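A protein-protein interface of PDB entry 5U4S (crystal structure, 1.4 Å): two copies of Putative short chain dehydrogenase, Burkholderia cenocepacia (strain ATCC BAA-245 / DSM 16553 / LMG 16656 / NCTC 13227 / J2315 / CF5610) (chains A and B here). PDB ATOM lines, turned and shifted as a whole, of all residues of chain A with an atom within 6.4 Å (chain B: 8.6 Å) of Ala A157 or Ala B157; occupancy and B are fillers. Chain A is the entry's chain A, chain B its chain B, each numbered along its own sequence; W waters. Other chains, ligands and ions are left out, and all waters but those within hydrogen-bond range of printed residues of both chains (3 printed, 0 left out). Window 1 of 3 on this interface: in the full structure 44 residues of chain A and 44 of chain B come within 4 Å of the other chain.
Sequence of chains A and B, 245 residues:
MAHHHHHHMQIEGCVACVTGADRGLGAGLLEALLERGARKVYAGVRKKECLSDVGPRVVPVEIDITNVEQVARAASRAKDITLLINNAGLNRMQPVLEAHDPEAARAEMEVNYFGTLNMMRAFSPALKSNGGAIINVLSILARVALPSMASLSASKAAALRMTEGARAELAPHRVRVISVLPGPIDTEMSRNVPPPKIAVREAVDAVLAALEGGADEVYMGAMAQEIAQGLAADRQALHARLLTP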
ATOM      1  N   LEU A 141       5.173  16.587  -0.974  1.00  0.00           N
ATOM      2  CA  LEU A 141       4.428  15.685  -1.854  1.00  0.00           C
ATOM      3  C   LEU A 141       5.124  14.343  -2.057  1.00  0.00           C
ATOM      4  O   LEU A 141       4.519  13.426  -2.624  1.00  0.00           O
ATOM      5  CB  LEU A 141       4.070  16.360  -3.179  1.00  0.00           C
ATOM      6  CG  LEU A 141       3.302  17.664  -2.977  1.00  0.00           C
ATOM      7  CD1 LEU A 141       2.918  18.243  -4.354  1.00  0.00           C
ATOM      8  CD2 LEU A 141       2.049  17.519  -2.084  1.00  0.00           C
ATOM      9  N   ALA A 142       6.342  14.166  -1.540  1.00  0.00           N
ATOM     10  CA  ALA A 142       6.896  12.814  -1.460  1.00  0.00           C
ATOM     11  C   ALA A 142       6.039  11.906  -0.599  1.00  0.00           C
ATOM     12  O   ALA A 142       6.116  10.686  -0.760  1.00  0.00           O
ATOM     13  CB  ALA A 142       8.292  12.856  -0.828  1.00  0.00           C
ATOM     14  N   ARG A 143       5.190  12.475   0.262  1.00  0.00           N
ATOM     15  CA  ARG A 143       4.392  11.673   1.182  1.00  0.00           C
ATOM     16  C   ARG A 143       2.928  11.527   0.800  1.00  0.00           C
ATOM     17  O   ARG A 143       2.262  10.632   1.331  1.00  0.00           O
ATOM     18  CB  ARG A 143       4.494  12.245   2.591  1.00  0.00           C
ATOM     19  CG  ARG A 143       5.981  12.221   3.022  1.00  0.00           C
ATOM     20  CD  ARG A 143       6.202  12.069   4.502  1.00  0.00           C
ATOM     21  NE  ARG A 143       5.323  11.058   5.062  1.00  0.00           N
ATOM     22  CZ  ARG A 143       4.907  11.112   6.310  1.00  0.00           C
ATOM     23  NH1 ARG A 143       5.292  12.107   7.110  1.00  0.00           N
ATOM     24  NH2 ARG A 143       4.081  10.173   6.759  1.00  0.00           N
ATOM     25  N   LEU A 152       4.774  14.672 -10.134  1.00  0.00           N
ATOM     26  CA  LEU A 152       5.843  15.262  -9.317  1.00  0.00           C
ATOM     27  C   LEU A 152       5.920  14.525  -7.989  1.00  0.00           C
ATOM     28  O   LEU A 152       7.003  14.117  -7.538  1.00  0.00           O
ATOM     29  CB  LEU A 152       5.569  16.752  -9.072  1.00  0.00           C
ATOM     30  CG  LEU A 152       6.458  17.520  -8.066  1.00  0.00           C
ATOM     31  CD1 LEU A 152       6.099  17.303  -6.585  1.00  0.00           C
ATOM     32  CD2 LEU A 152       7.973  17.318  -8.311  1.00  0.00           C
ATOM     33  N   SER A 153       4.754  14.303  -7.364  1.00  0.00           N
ATOM     34  CA  SER A 153       4.696  13.592  -6.094  1.00  0.00           C
ATOM     35  C   SER A 153       5.374  12.230  -6.195  1.00  0.00           C
ATOM     36  O   SER A 153       6.198  11.874  -5.349  1.00  0.00           O
ATOM     37  CB  SER A 153       3.213  13.459  -5.744  1.00  0.00           C
ATOM     38  OG  SER A 153       3.002  12.659  -4.596  1.00  0.00           O
ATOM     39  N   ALA A 154       5.047  11.472  -7.241  1.00  0.00           N
ATOM     40  CA  ALA A 154       5.655  10.152  -7.437  1.00  0.00           C
ATOM     41  C   ALA A 154       7.183  10.226  -7.521  1.00  0.00           C
ATOM     42  O   ALA A 154       7.882   9.400  -6.914  1.00  0.00           O
ATOM     43  CB  ALA A 154       5.067   9.460  -8.677  1.00  0.00           C
ATOM     44  N   SER A 155       7.718  11.181  -8.284  1.00  0.00           N
ATOM     45  CA  SER A 155       9.179  11.274  -8.402  1.00  0.00           C
ATOM     46  C   SER A 155       9.833  11.640  -7.071  1.00  0.00           C
ATOM     47  O   SER A 155      10.936  11.165  -6.764  1.00  0.00           O
ATOM     48  CB  SER A 155       9.561  12.278  -9.506  1.00  0.00           C
ATOM     49  OG  SER A 155       9.261  13.633  -9.166  1.00  0.00           O
ATOM     50  N   LYS A 156       9.162  12.469  -6.265  1.00  0.00           N
ATOM     51  CA  LYS A 156       9.742  12.836  -4.977  1.00  0.00           C
ATOM     52  C   LYS A 156       9.620  11.702  -3.961  1.00  0.00           C
ATOM     53  O   LYS A 156      10.505  11.560  -3.104  1.00  0.00           O
ATOM     54  CB  LYS A 156       9.138  14.156  -4.477  1.00  0.00           C
ATOM     55  CG  LYS A 156       9.513  15.387  -5.327  1.00  0.00           C
ATOM     56  CD  LYS A 156      10.934  15.845  -5.037  1.00  0.00           C
ATOM     57  CE  LYS A 156      11.143  17.215  -5.690  1.00  0.00           C
ATOM     58  NZ  LYS A 156      12.489  17.836  -5.385  1.00  0.00           N
ATOM     59  N   ALA A 157       8.547  10.895  -4.027  1.00  0.00           N
ATOM     60  CA  ALA A 157       8.427   9.711  -3.172  1.00  0.00           C
ATOM     61  C   ALA A 157       9.516   8.700  -3.491  1.00  0.00           C
ATOM     62  O   ALA A 157      10.124   8.105  -2.584  1.00  0.00           O
ATOM     63  CB  ALA A 157       7.048   9.092  -3.411  1.00  0.00           C
ATOM     64  N   ALA A 158       9.782   8.486  -4.794  1.00  0.00           N
ATOM     65  CA  ALA A 158      10.914   7.646  -5.184  1.00  0.00           C
ATOM     66  C   ALA A 158      12.202   8.168  -4.561  1.00  0.00           C
ATOM     67  O   ALA A 158      12.996   7.396  -4.005  1.00  0.00           O
ATOM     68  CB  ALA A 158      11.017   7.587  -6.716  1.00  0.00           C
ATOM     69  N   ALA A 159      12.426   9.482  -4.655  1.00  0.00           N
ATOM     70  CA  ALA A 159      13.647  10.069  -4.101  1.00  0.00           C
ATOM     71  C   ALA A 159      13.708   9.922  -2.583  1.00  0.00           C
ATOM     72  O   ALA A 159      14.808   9.785  -2.027  1.00  0.00           O
ATOM     73  CB  ALA A 159      13.753  11.533  -4.535  1.00  0.00           C
ATOM     74  N   LEU A 160      12.565   9.954  -1.895  1.00  0.00           N
ATOM     75  CA  LEU A 160      12.564   9.768  -0.442  1.00  0.00           C
ATOM     76  C   LEU A 160      12.965   8.350  -0.046  1.00  0.00           C
ATOM     77  O   LEU A 160      13.790   8.164   0.853  1.00  0.00           O
ATOM     78  CB  LEU A 160      11.207  10.164   0.164  1.00  0.00           C
ATOM     79  CG  LEU A 160      11.103  10.067   1.691  1.00  0.00           C
ATOM     80  CD1 LEU A 160      12.185  10.903   2.413  1.00  0.00           C
ATOM     81  CD2 LEU A 160       9.713  10.528   2.150  1.00  0.00           C
ATOM     82  N   ARG A 161      12.402   7.323  -0.699  1.00  0.00           N
ATOM     83  CA  ARG A 161      12.845   5.954  -0.422  1.00  0.00           C
ATOM     84  C   ARG A 161      14.331   5.795  -0.733  1.00  0.00           C
ATOM     85  O   ARG A 161      15.064   5.127  -0.001  1.00  0.00           O
ATOM     86  CB  ARG A 161      12.035   4.923  -1.232  1.00  0.00           C
ATOM     87  CG  ARG A 161      10.506   4.884  -0.993  1.00  0.00           C
ATOM     88  CD  ARG A 161      10.103   4.362   0.401  1.00  0.00           C
ATOM     89  NE  ARG A 161      10.101   5.431   1.407  1.00  0.00           N
ATOM     90  CZ  ARG A 161       9.121   6.326   1.563  1.00  0.00           C
ATOM     91  NH1 ARG A 161       8.010   6.271   0.818  1.00  0.00           N
ATOM     92  NH2 ARG A 161       9.240   7.288   2.487  1.00  0.00           N
ATOM     93  N   MET A 162      14.778   6.380  -1.844  1.00  0.00           N
ATOM     94  CA  MET A 162      16.196   6.313  -2.182  1.00  0.00           C
ATOM     95  C   MET A 162      17.049   6.981  -1.111  1.00  0.00           C
ATOM     96  O   MET A 162      18.116   6.457  -0.768  1.00  0.00           O
ATOM     97  CB  MET A 162      16.415   6.933  -3.566  1.00  0.00           C
ATOM     98  CG  MET A 162      17.889   6.990  -4.019  1.00  0.00           C
ATOM     99  SD  MET A 162      18.798   8.435  -3.410  1.00  0.00           S
ATOM    100  CE  MET A 162      18.036   9.742  -4.365  1.00  0.00           C
ATOM    101  N   MET B 109      11.729   0.807 -11.969  1.00  0.00           N
ATOM    102  CA  MET B 109      10.832   1.936 -12.182  1.00  0.00           C
ATOM    103  C   MET B 109      10.036   1.758 -13.472  1.00  0.00           C
ATOM    104  O   MET B 109       8.838   2.066 -13.521  1.00  0.00           O
ATOM    105  CB  MET B 109      11.646   3.236 -12.180  1.00  0.00           C
ATOM    106  CG  MET B 109      10.802   4.501 -12.091  1.00  0.00           C
ATOM    107  SD  MET B 109       9.905   4.651 -10.518  1.00  0.00           S
ATOM    108  CE  MET B 109      11.255   4.984  -9.367  1.00  0.00           C
ATOM    109  N   ASN B 112       7.312  -1.133 -12.494  1.00  0.00           N
ATOM    110  CA  ASN B 112       6.403  -0.967 -11.367  1.00  0.00           C
ATOM    111  C   ASN B 112       5.714   0.385 -11.382  1.00  0.00           C
ATOM    112  O   ASN B 112       4.594   0.509 -10.847  1.00  0.00           O
ATOM    113  CB  ASN B 112       7.142  -1.156 -10.041  1.00  0.00           C
ATOM    114  CG  ASN B 112       7.802  -2.510  -9.931  1.00  0.00           C
ATOM    115  OD1 ASN B 112       7.367  -3.496 -10.545  1.00  0.00           O
ATOM    116  ND2 ASN B 112       8.872  -2.569  -9.163  1.00  0.00           N
ATOM    117  N   TYR B 113       6.350   1.413 -11.965  1.00  0.00           N
ATOM    118  CA  TYR B 113       5.728   2.729 -12.079  1.00  0.00           C
ATOM    119  C   TYR B 113       5.233   2.996 -13.497  1.00  0.00           C
ATOM    120  O   TYR B 113       4.024   3.116 -13.721  1.00  0.00           O
ATOM    121  CB  TYR B 113       6.725   3.813 -11.645  1.00  0.00           C
ATOM    122  CG  TYR B 113       6.215   5.227 -11.790  1.00  0.00           C
ATOM    123  CD1 TYR B 113       5.116   5.680 -11.054  1.00  0.00           C
ATOM    124  CD2 TYR B 113       6.840   6.126 -12.653  1.00  0.00           C
ATOM    125  CE1 TYR B 113       4.679   6.986 -11.146  1.00  0.00           C
ATOM    126  CE2 TYR B 113       6.400   7.452 -12.767  1.00  0.00           C
ATOM    127  CZ  TYR B 113       5.316   7.884 -12.004  1.00  0.00           C
ATOM    128  OH  TYR B 113       4.868   9.189 -12.080  1.00  0.00           O
ATOM    129  N   LEU B 138       1.089  -3.315  -4.765  1.00  0.00           N
ATOM    130  CA  LEU B 138       2.283  -2.501  -4.535  1.00  0.00           C
ATOM    131  C   LEU B 138       3.221  -3.290  -3.625  1.00  0.00           C
ATOM    132  O   LEU B 138       3.616  -4.397  -3.997  1.00  0.00           O
ATOM    133  CB  LEU B 138       1.875  -1.118  -4.013  1.00  0.00           C
ATOM    134  CG  LEU B 138       0.938  -0.384  -4.986  1.00  0.00           C
ATOM    135  CD1 LEU B 138       0.761   1.057  -4.510  1.00  0.00           C
ATOM    136  CD2 LEU B 138       1.457  -0.395  -6.401  1.00  0.00           C
ATOM    137  N   SER B 139       3.591  -2.752  -2.456  1.00  0.00           N
ATOM    138  CA  SER B 139       4.482  -3.403  -1.500  1.00  0.00           C
ATOM    139  C   SER B 139       4.446  -2.553  -0.242  1.00  0.00           C
ATOM    140  O   SER B 139       4.289  -1.331  -0.331  1.00  0.00           O
ATOM    141  CB  SER B 139       5.937  -3.427  -2.027  1.00  0.00           C
ATOM    142  OG  SER B 139       6.811  -3.906  -0.996  1.00  0.00           O
ATOM    143  N   ILE B 140       4.635  -3.186   0.922  1.00  0.00           N
ATOM    144  CA  ILE B 140       4.880  -2.376   2.122  1.00  0.00           C
ATOM    145  C   ILE B 140       6.073  -1.444   1.941  1.00  0.00           C
ATOM    146  O   ILE B 140       6.138  -0.378   2.576  1.00  0.00           O
ATOM    147  CB  ILE B 140       4.984  -3.250   3.400  1.00  0.00           C
ATOM    148  CG1 ILE B 140       5.066  -2.383   4.670  1.00  0.00           C
ATOM    149  CG2 ILE B 140       6.192  -4.174   3.349  1.00  0.00           C
ATOM    150  CD1 ILE B 140       3.865  -1.473   4.863  1.00  0.00           C
ATOM    151  N   LEU B 141       7.030  -1.819   1.087  1.00  0.00           N
ATOM    152  CA  LEU B 141       8.190  -0.969   0.855  1.00  0.00           C
ATOM    153  C   LEU B 141       7.845   0.304   0.097  1.00  0.00           C
ATOM    154  O   LEU B 141       8.687   1.202   0.018  1.00  0.00           O
ATOM    155  CB  LEU B 141       9.295  -1.777   0.172  1.00  0.00           C
ATOM    156  CG  LEU B 141       9.695  -3.037   0.961  1.00  0.00           C
ATOM    157  CD1 LEU B 141      10.889  -3.732   0.288  1.00  0.00           C
ATOM    158  CD2 LEU B 141      10.033  -2.728   2.417  1.00  0.00           C
ATOM    159  N   ALA B 142       6.607   0.458  -0.380  1.00  0.00           N
ATOM    160  CA  ALA B 142       6.183   1.789  -0.811  1.00  0.00           C
ATOM    161  C   ALA B 142       6.227   2.812   0.321  1.00  0.00           C
ATOM    162  O   ALA B 142       6.298   4.012   0.046  1.00  0.00           O
ATOM    163  CB  ALA B 142       4.765   1.733  -1.397  1.00  0.00           C
ATOM    164  N   ARG B 143       6.186   2.367   1.578  1.00  0.00           N
ATOM    165  CA  ARG B 143       6.158   3.253   2.747  1.00  0.00           C
ATOM    166  C   ARG B 143       7.521   3.470   3.396  1.00  0.00           C
ATOM    167  O   ARG B 143       7.681   4.455   4.117  1.00  0.00           O
ATOM    168  CB  ARG B 143       5.232   2.702   3.845  1.00  0.00           C
ATOM    169  CG  ARG B 143       3.806   2.328   3.492  1.00  0.00           C
ATOM    170  CD  ARG B 143       2.817   3.494   3.409  1.00  0.00           C
ATOM    171  NE  ARG B 143       3.013   4.585   4.376  1.00  0.00           N
ATOM    172  CZ  ARG B 143       2.472   4.677   5.593  1.00  0.00           C
ATOM    173  NH1 ARG B 143       1.703   3.742   6.134  1.00  0.00           N
ATOM    174  NH2 ARG B 143       2.761   5.763   6.303  1.00  0.00           N
ATOM    175  N   VAL B 144       8.483   2.571   3.204  1.00  0.00           N
ATOM    176  CA  VAL B 144       9.795   2.667   3.860  1.00  0.00           C
ATOM    177  C   VAL B 144      10.753   1.779   3.076  1.00  0.00           C
ATOM    178  O   VAL B 144      10.378   0.686   2.643  1.00  0.00           O
ATOM    179  CB  VAL B 144       9.715   2.277   5.357  1.00  0.00           C
ATOM    180  CG1 VAL B 144       9.310   0.806   5.507  1.00  0.00           C
ATOM    181  CG2 VAL B 144      11.048   2.583   6.067  1.00  0.00           C
ATOM    182  N   ALA B 145      11.983   2.257   2.877  1.00  0.00           N
ATOM    183  CA  ALA B 145      12.965   1.435   2.185  1.00  0.00           C
ATOM    184  C   ALA B 145      13.481   0.318   3.079  1.00  0.00           C
ATOM    185  O   ALA B 145      13.676   0.501   4.283  1.00  0.00           O
ATOM    186  CB  ALA B 145      14.136   2.311   1.749  1.00  0.00           C
ATOM    187  N   ALA B 150      16.316  -1.019  -1.965  1.00  0.00           N
ATOM    188  CA  ALA B 150      15.783   0.334  -1.868  1.00  0.00           C
ATOM    189  C   ALA B 150      15.280   0.852  -3.210  1.00  0.00           C
ATOM    190  O   ALA B 150      14.384   1.707  -3.238  1.00  0.00           O
ATOM    191  CB  ALA B 150      16.796   1.305  -1.248  1.00  0.00           C
ATOM    192  N   SER B 151      15.851   0.373  -4.326  1.00  0.00           N
ATOM    193  CA  SER B 151      15.334   0.811  -5.625  1.00  0.00           C
ATOM    194  C   SER B 151      13.976   0.188  -5.947  1.00  0.00           C
ATOM    195  O   SER B 151      13.141   0.835  -6.601  1.00  0.00           O
ATOM    196  CB  SER B 151      16.354   0.607  -6.757  1.00  0.00           C
ATOM    197  OG  SER B 151      16.821  -0.730  -6.847  1.00  0.00           O
ATOM    198  N   LEU B 152      13.718  -1.041  -5.486  1.00  0.00           N
ATOM    199  CA  LEU B 152      12.356  -1.568  -5.586  1.00  0.00           C
ATOM    200  C   LEU B 152      11.420  -0.693  -4.765  1.00  0.00           C
ATOM    201  O   LEU B 152      10.343  -0.288  -5.227  1.00  0.00           O
ATOM    202  CB  LEU B 152      12.340  -3.019  -5.070  1.00  0.00           C
ATOM    203  CG  LEU B 152      10.979  -3.733  -4.897  1.00  0.00           C
ATOM    204  CD1 LEU B 152      10.217  -3.302  -3.640  1.00  0.00           C
ATOM    205  CD2 LEU B 152      10.083  -3.666  -6.144  1.00  0.00           C
ATOM    206  N   SER B 153      11.844  -0.374  -3.538  1.00  0.00           N
ATOM    207  CA  SER B 153      11.051   0.474  -2.661  1.00  0.00           C
ATOM    208  C   SER B 153      10.682   1.790  -3.347  1.00  0.00           C
ATOM    209  O   SER B 153       9.508   2.204  -3.350  1.00  0.00           O
ATOM    210  CB  SER B 153      11.840   0.706  -1.367  1.00  0.00           C
ATOM    211  OG  SER B 153      11.209   1.672  -0.527  1.00  0.00           O
ATOM    212  N   ALA B 154      11.679   2.465  -3.942  1.00  0.00           N
ATOM    213  CA  ALA B 154      11.419   3.730  -4.628  1.00  0.00           C
ATOM    214  C   ALA B 154      10.372   3.574  -5.727  1.00  0.00           C
ATOM    215  O   ALA B 154       9.494   4.436  -5.874  1.00  0.00           O
ATOM    216  CB  ALA B 154      12.720   4.259  -5.219  1.00  0.00           C
ATOM    217  N   SER B 155      10.453   2.481  -6.516  1.00  0.00           N
ATOM    218  CA  SER B 155       9.498   2.306  -7.611  1.00  0.00           C
ATOM    219  C   SER B 155       8.088   2.075  -7.096  1.00  0.00           C
ATOM    220  O   SER B 155       7.117   2.537  -7.719  1.00  0.00           O
ATOM    221  CB  SER B 155       9.955   1.180  -8.553  1.00  0.00           C
ATOM    222  OG  SER B 155       9.830  -0.116  -7.947  1.00  0.00           O
ATOM    223  N   LYS B 156       7.949   1.385  -5.960  1.00  0.00           N
ATOM    224  CA  LYS B 156       6.619   1.127  -5.398  1.00  0.00           C
ATOM    225  C   LYS B 156       6.049   2.367  -4.722  1.00  0.00           C
ATOM    226  O   LYS B 156       4.830   2.571  -4.746  1.00  0.00           O
ATOM    227  CB  LYS B 156       6.675  -0.078  -4.445  1.00  0.00           C
ATOM    228  CG  LYS B 156       6.965  -1.417  -5.155  1.00  0.00           C
ATOM    229  CD  LYS B 156       5.735  -1.933  -5.949  1.00  0.00           C
ATOM    230  CE  LYS B 156       6.005  -3.380  -6.402  1.00  0.00           C
ATOM    231  NZ  LYS B 156       4.798  -3.965  -7.089  1.00  0.00           N
ATOM    232  N   ALA B 157       6.910   3.212  -4.138  1.00  0.00           N
ATOM    233  CA  ALA B 157       6.443   4.484  -3.593  1.00  0.00           C
ATOM    234  C   ALA B 157       5.942   5.413  -4.687  1.00  0.00           C
ATOM    235  O   ALA B 157       4.909   6.085  -4.521  1.00  0.00           O
ATOM    236  CB  ALA B 157       7.579   5.134  -2.793  1.00  0.00           C
ATOM    237  N   ALA B 158       6.675   5.473  -5.808  1.00  0.00           N
ATOM    238  CA  ALA B 158       6.187   6.237  -6.952  1.00  0.00           C
ATOM    239  C   ALA B 158       4.822   5.711  -7.377  1.00  0.00           C
ATOM    240  O   ALA B 158       3.894   6.494  -7.634  1.00  0.00           O
ATOM    241  CB  ALA B 158       7.176   6.109  -8.115  1.00  0.00           C
ATOM    242  N   ALA B 159       4.678   4.377  -7.435  1.00  0.00           N
ATOM    243  CA  ALA B 159       3.398   3.799  -7.835  1.00  0.00           C
ATOM    244  C   ALA B 159       2.289   4.121  -6.833  1.00  0.00           C
ATOM    245  O   ALA B 159       1.128   4.288  -7.244  1.00  0.00           O
ATOM    246  CB  ALA B 159       3.544   2.285  -7.984  1.00  0.00           C
ATOM    247  N   LEU B 160       2.606   4.250  -5.539  1.00  0.00           N
ATOM    248  CA  LEU B 160       1.585   4.591  -4.554  1.00  0.00           C
ATOM    249  C   LEU B 160       1.090   6.027  -4.729  1.00  0.00           C
ATOM    250  O   LEU B 160      -0.126   6.277  -4.701  1.00  0.00           O
ATOM    251  CB  LEU B 160       2.103   4.339  -3.128  1.00  0.00           C
ATOM    252  CG  LEU B 160       1.109   4.615  -1.994  1.00  0.00           C
ATOM    253  CD1 LEU B 160      -0.219   3.814  -2.123  1.00  0.00           C
ATOM    254  CD2 LEU B 160       1.760   4.309  -0.638  1.00  0.00           C
ATOM    255  N   ARG B 161       2.004   6.987  -4.947  1.00  0.00           N
ATOM    256  CA  ARG B 161       1.560   8.350  -5.230  1.00  0.00           C
ATOM    257  C   ARG B 161       0.726   8.388  -6.498  1.00  0.00           C
ATOM    258  O   ARG B 161      -0.282   9.102  -6.561  1.00  0.00           O
ATOM    259  CB  ARG B 161       2.756   9.302  -5.376  1.00  0.00           C
ATOM    260  CG  ARG B 161       3.648   9.458  -4.136  1.00  0.00           C
ATOM    261  CD  ARG B 161       3.008  10.179  -2.945  1.00  0.00           C
ATOM    262  NE  ARG B 161       2.226   9.270  -2.098  1.00  0.00           N
ATOM    263  CZ  ARG B 161       2.771   8.441  -1.207  1.00  0.00           C
ATOM    264  NH1 ARG B 161       4.079   8.422  -0.996  1.00  0.00           N
ATOM    265  NH2 ARG B 161       1.987   7.622  -0.506  1.00  0.00           N
ATOM    266  N   MET B 162       1.164   7.658  -7.529  1.00  0.00           N
ATOM    267  CA  MET B 162       0.394   7.600  -8.760  1.00  0.00           C
ATOM    268  C   MET B 162      -1.005   7.047  -8.512  1.00  0.00           C
ATOM    269  O   MET B 162      -1.987   7.561  -9.082  1.00  0.00           O
ATOM    270  CB  MET B 162       1.186   6.799  -9.802  1.00  0.00           C
ATOM    271  CG  MET B 162       0.479   6.591 -11.161  1.00  0.00           C
ATOM    272  SD  MET B 162      -0.712   5.236 -11.180  1.00  0.00           S
ATOM    273  CE  MET B 162       0.331   3.816 -10.903  1.00  0.00           C
ATOM    274  N   THR B 163      -1.119   6.023  -7.669  1.00  0.00           N
ATOM    275  CA  THR B 163      -2.434   5.433  -7.378  1.00  0.00           C
ATOM    276  C   THR B 163      -3.345   6.449  -6.689  1.00  0.00           C
ATOM    277  O   THR B 163      -4.542   6.535  -6.996  1.00  0.00           O
ATOM    278  CB  THR B 163      -2.251   4.158  -6.549  1.00  0.00           C
ATOM    279  OG1 THR B 163      -1.429   3.225  -7.265  1.00  0.00           O
ATOM    280  CG2 THR B 163      -3.593   3.462  -6.239  1.00  0.00           C
ATOM    281  N   GLU B 164      -2.781   7.247  -5.769  1.00  0.00           N
ATOM    282  CA  GLU B 164      -3.544   8.307  -5.120  1.00  0.00           C
ATOM    283  C   GLU B 164      -4.056   9.322  -6.126  1.00  0.00           C
ATOM    284  O   GLU B 164      -5.224   9.721  -6.082  1.00  0.00           O
ATOM    285  CB  GLU B 164      -2.681   8.986  -4.051  1.00  0.00           C
ATOM    286  CG  GLU B 164      -2.344   8.059  -2.871  1.00  0.00           C
ATOM    287  CD  GLU B 164      -1.177   8.546  -2.020  1.00  0.00           C
ATOM    288  OE1 GLU B 164      -0.565   9.600  -2.339  1.00  0.00           O
ATOM    289  OE2 GLU B 164      -0.873   7.871  -1.023  1.00  0.00           O
ATOM    290  N   LEU B 181      -0.693  -3.461  -0.149  1.00  0.00           N
ATOM    291  CA  LEU B 181       0.712  -3.320   0.240  1.00  0.00           C
ATOM    292  C   LEU B 181       1.149  -4.556   1.014  1.00  0.00           C
ATOM    293  O   LEU B 181       1.030  -4.584   2.246  1.00  0.00           O
ATOM    294  CB  LEU B 181       0.926  -2.061   1.086  1.00  0.00           C
ATOM    295  CG  LEU B 181       0.641  -0.723   0.373  1.00  0.00           C
ATOM    296  CD1 LEU B 181      -0.848  -0.350   0.462  1.00  0.00           C
ATOM    297  CD2 LEU B 181       1.465   0.391   0.972  1.00  0.00           C
HETATM  298  O   HOH W   1       4.535   6.184   0.733  1.00  0.00           O
HETATM  299  O   HOH W   2       9.653   5.872   5.517  1.00  0.00           O
HETATM  300  O   HOH W   3      -0.336   9.294   1.283  1.00  0.00           O
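Among the printed residues, merely in contact across the chains: Ser A153 with Arg B161, Arg A161 with Ser B153, Ala A154 with Ala B158, Ala A158 with Ala B154, Arg A143 with Arg B161, Ala A154 with Tyr B113, Arg A161 with Ala B145, Arg A161 with Ala B157, Arg A161 with Arg B143, Arg A161 with Leu B141, Ala A157 with Arg B161, Leu A141 with Arg B161, Arg A161 with Ala B154, Ala A154 with Arg B161, Arg A161 with Val B144, Ala A158 with Met B109 and Ala A157 with Ala B157.
Ala A142 touches Arg B161, and with the chains exchanged Arg A161 touches Ala B142. Ser A153 touches Arg B161, and with the chains exchanged Arg A161 touches Ser B153. Ala A154 touches Ala B158, and with the chains exchanged Ala A158 touches Ala B154. Ala A157 touches its own counterpart, Ala B157. Of the 19 pairs that touch across the chains among the printed residues, 15 have their exchanged pair printed and touching as well.
The side-chain hydroxyl of Ser B139 lies within hydrogen-bond range of the backbone NH of Leu B141 (3.0 Å). O of Leu B141 lies within hydrogen-bond range of OG of Ser B153 (2.6 Å). The backbone carbonyl oxygen (O) of Val B144 lies within hydrogen-bond range of the side-chain hydroxyl (OG) of Ser B153, at 3.4 Å. OE1 of Glu B164 lies within salt-bridge range of NE of Arg B161, 2.8 Å away. OG of Ser A153 sits at hydrogen-bond distance from O of Leu A141 (2.6 Å).
Along chain B the printed residues that touch a printed residue of chain A span positions 109 to 161. Of the 14 printed residues of chain A, 8 touch a printed residue of chain B. Hydrophobic or aromatic side chains of chain A that line the printed part of chain B: Ala A154, Ala A157 and Ala A158. Among the printed residues, no Asp or Glu carboxylate lies within 4 Å of a Lys or Arg side-chain nitrogen of the other chain.
Water W3 lies within hydrogen-bond range of OE2 of Glu B164 (2.8 Å), O of Arg A143 (2.9 Å) and NH2 of Arg B161 (3.4 Å). Water W2 bridges the backbone carbonyl oxygen (O) of Arg B143 (2.8 Å) and the guanidinium group (NH2) of Arg A161 (3.4 Å). Water W1 lies within hydrogen-bond range of NH1 of Arg B161 (2.9 Å), O of Ala B142 (2.9 Å) and NH1 of Arg A161 (3.5 Å).
Of chain B, only Ala B157 and Arg B161 come within 4 Å of Ala A157. Ala B157 touches two residues of chain A. Of the printed residues of chain A, Val B144 touches Arg A161 (3.7 Å). Printed residues of chain B within 4 Å of Ala A142: Arg B161 (3.1 Å). Of the printed residues of chain A, Ala B142 touches Arg A161. Of the printed residues of chain B, Ser A153 touches Arg B161 (3.0 Å). Of the printed residues of chain A, Arg B161 touches Leu A141 (3.6 Å), Ala A142 (3.1 Å), Arg A143 (3.4 Å), Ser A153 (3.0 Å), Ala A154 (3.7 Å) and Ala A157 (3.5 Å). The nearest residue of chain B that does not touch Ala A157 is Ala B158 (4.4 Å). The nearest residue of chain A that does not touch Ala B157 is Ala A158 (4.5 Å).
The guanidinium group of Arg A161 sits at hydrogen-bond distance from the backbone carbonyl oxygen of Ala B142 (2.9 Å). The backbone carbonyl oxygen (O) of Ala A142 is in hydrogen-bond range of the guanidinium group (NH1) of Arg B161 (3.1 Å).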
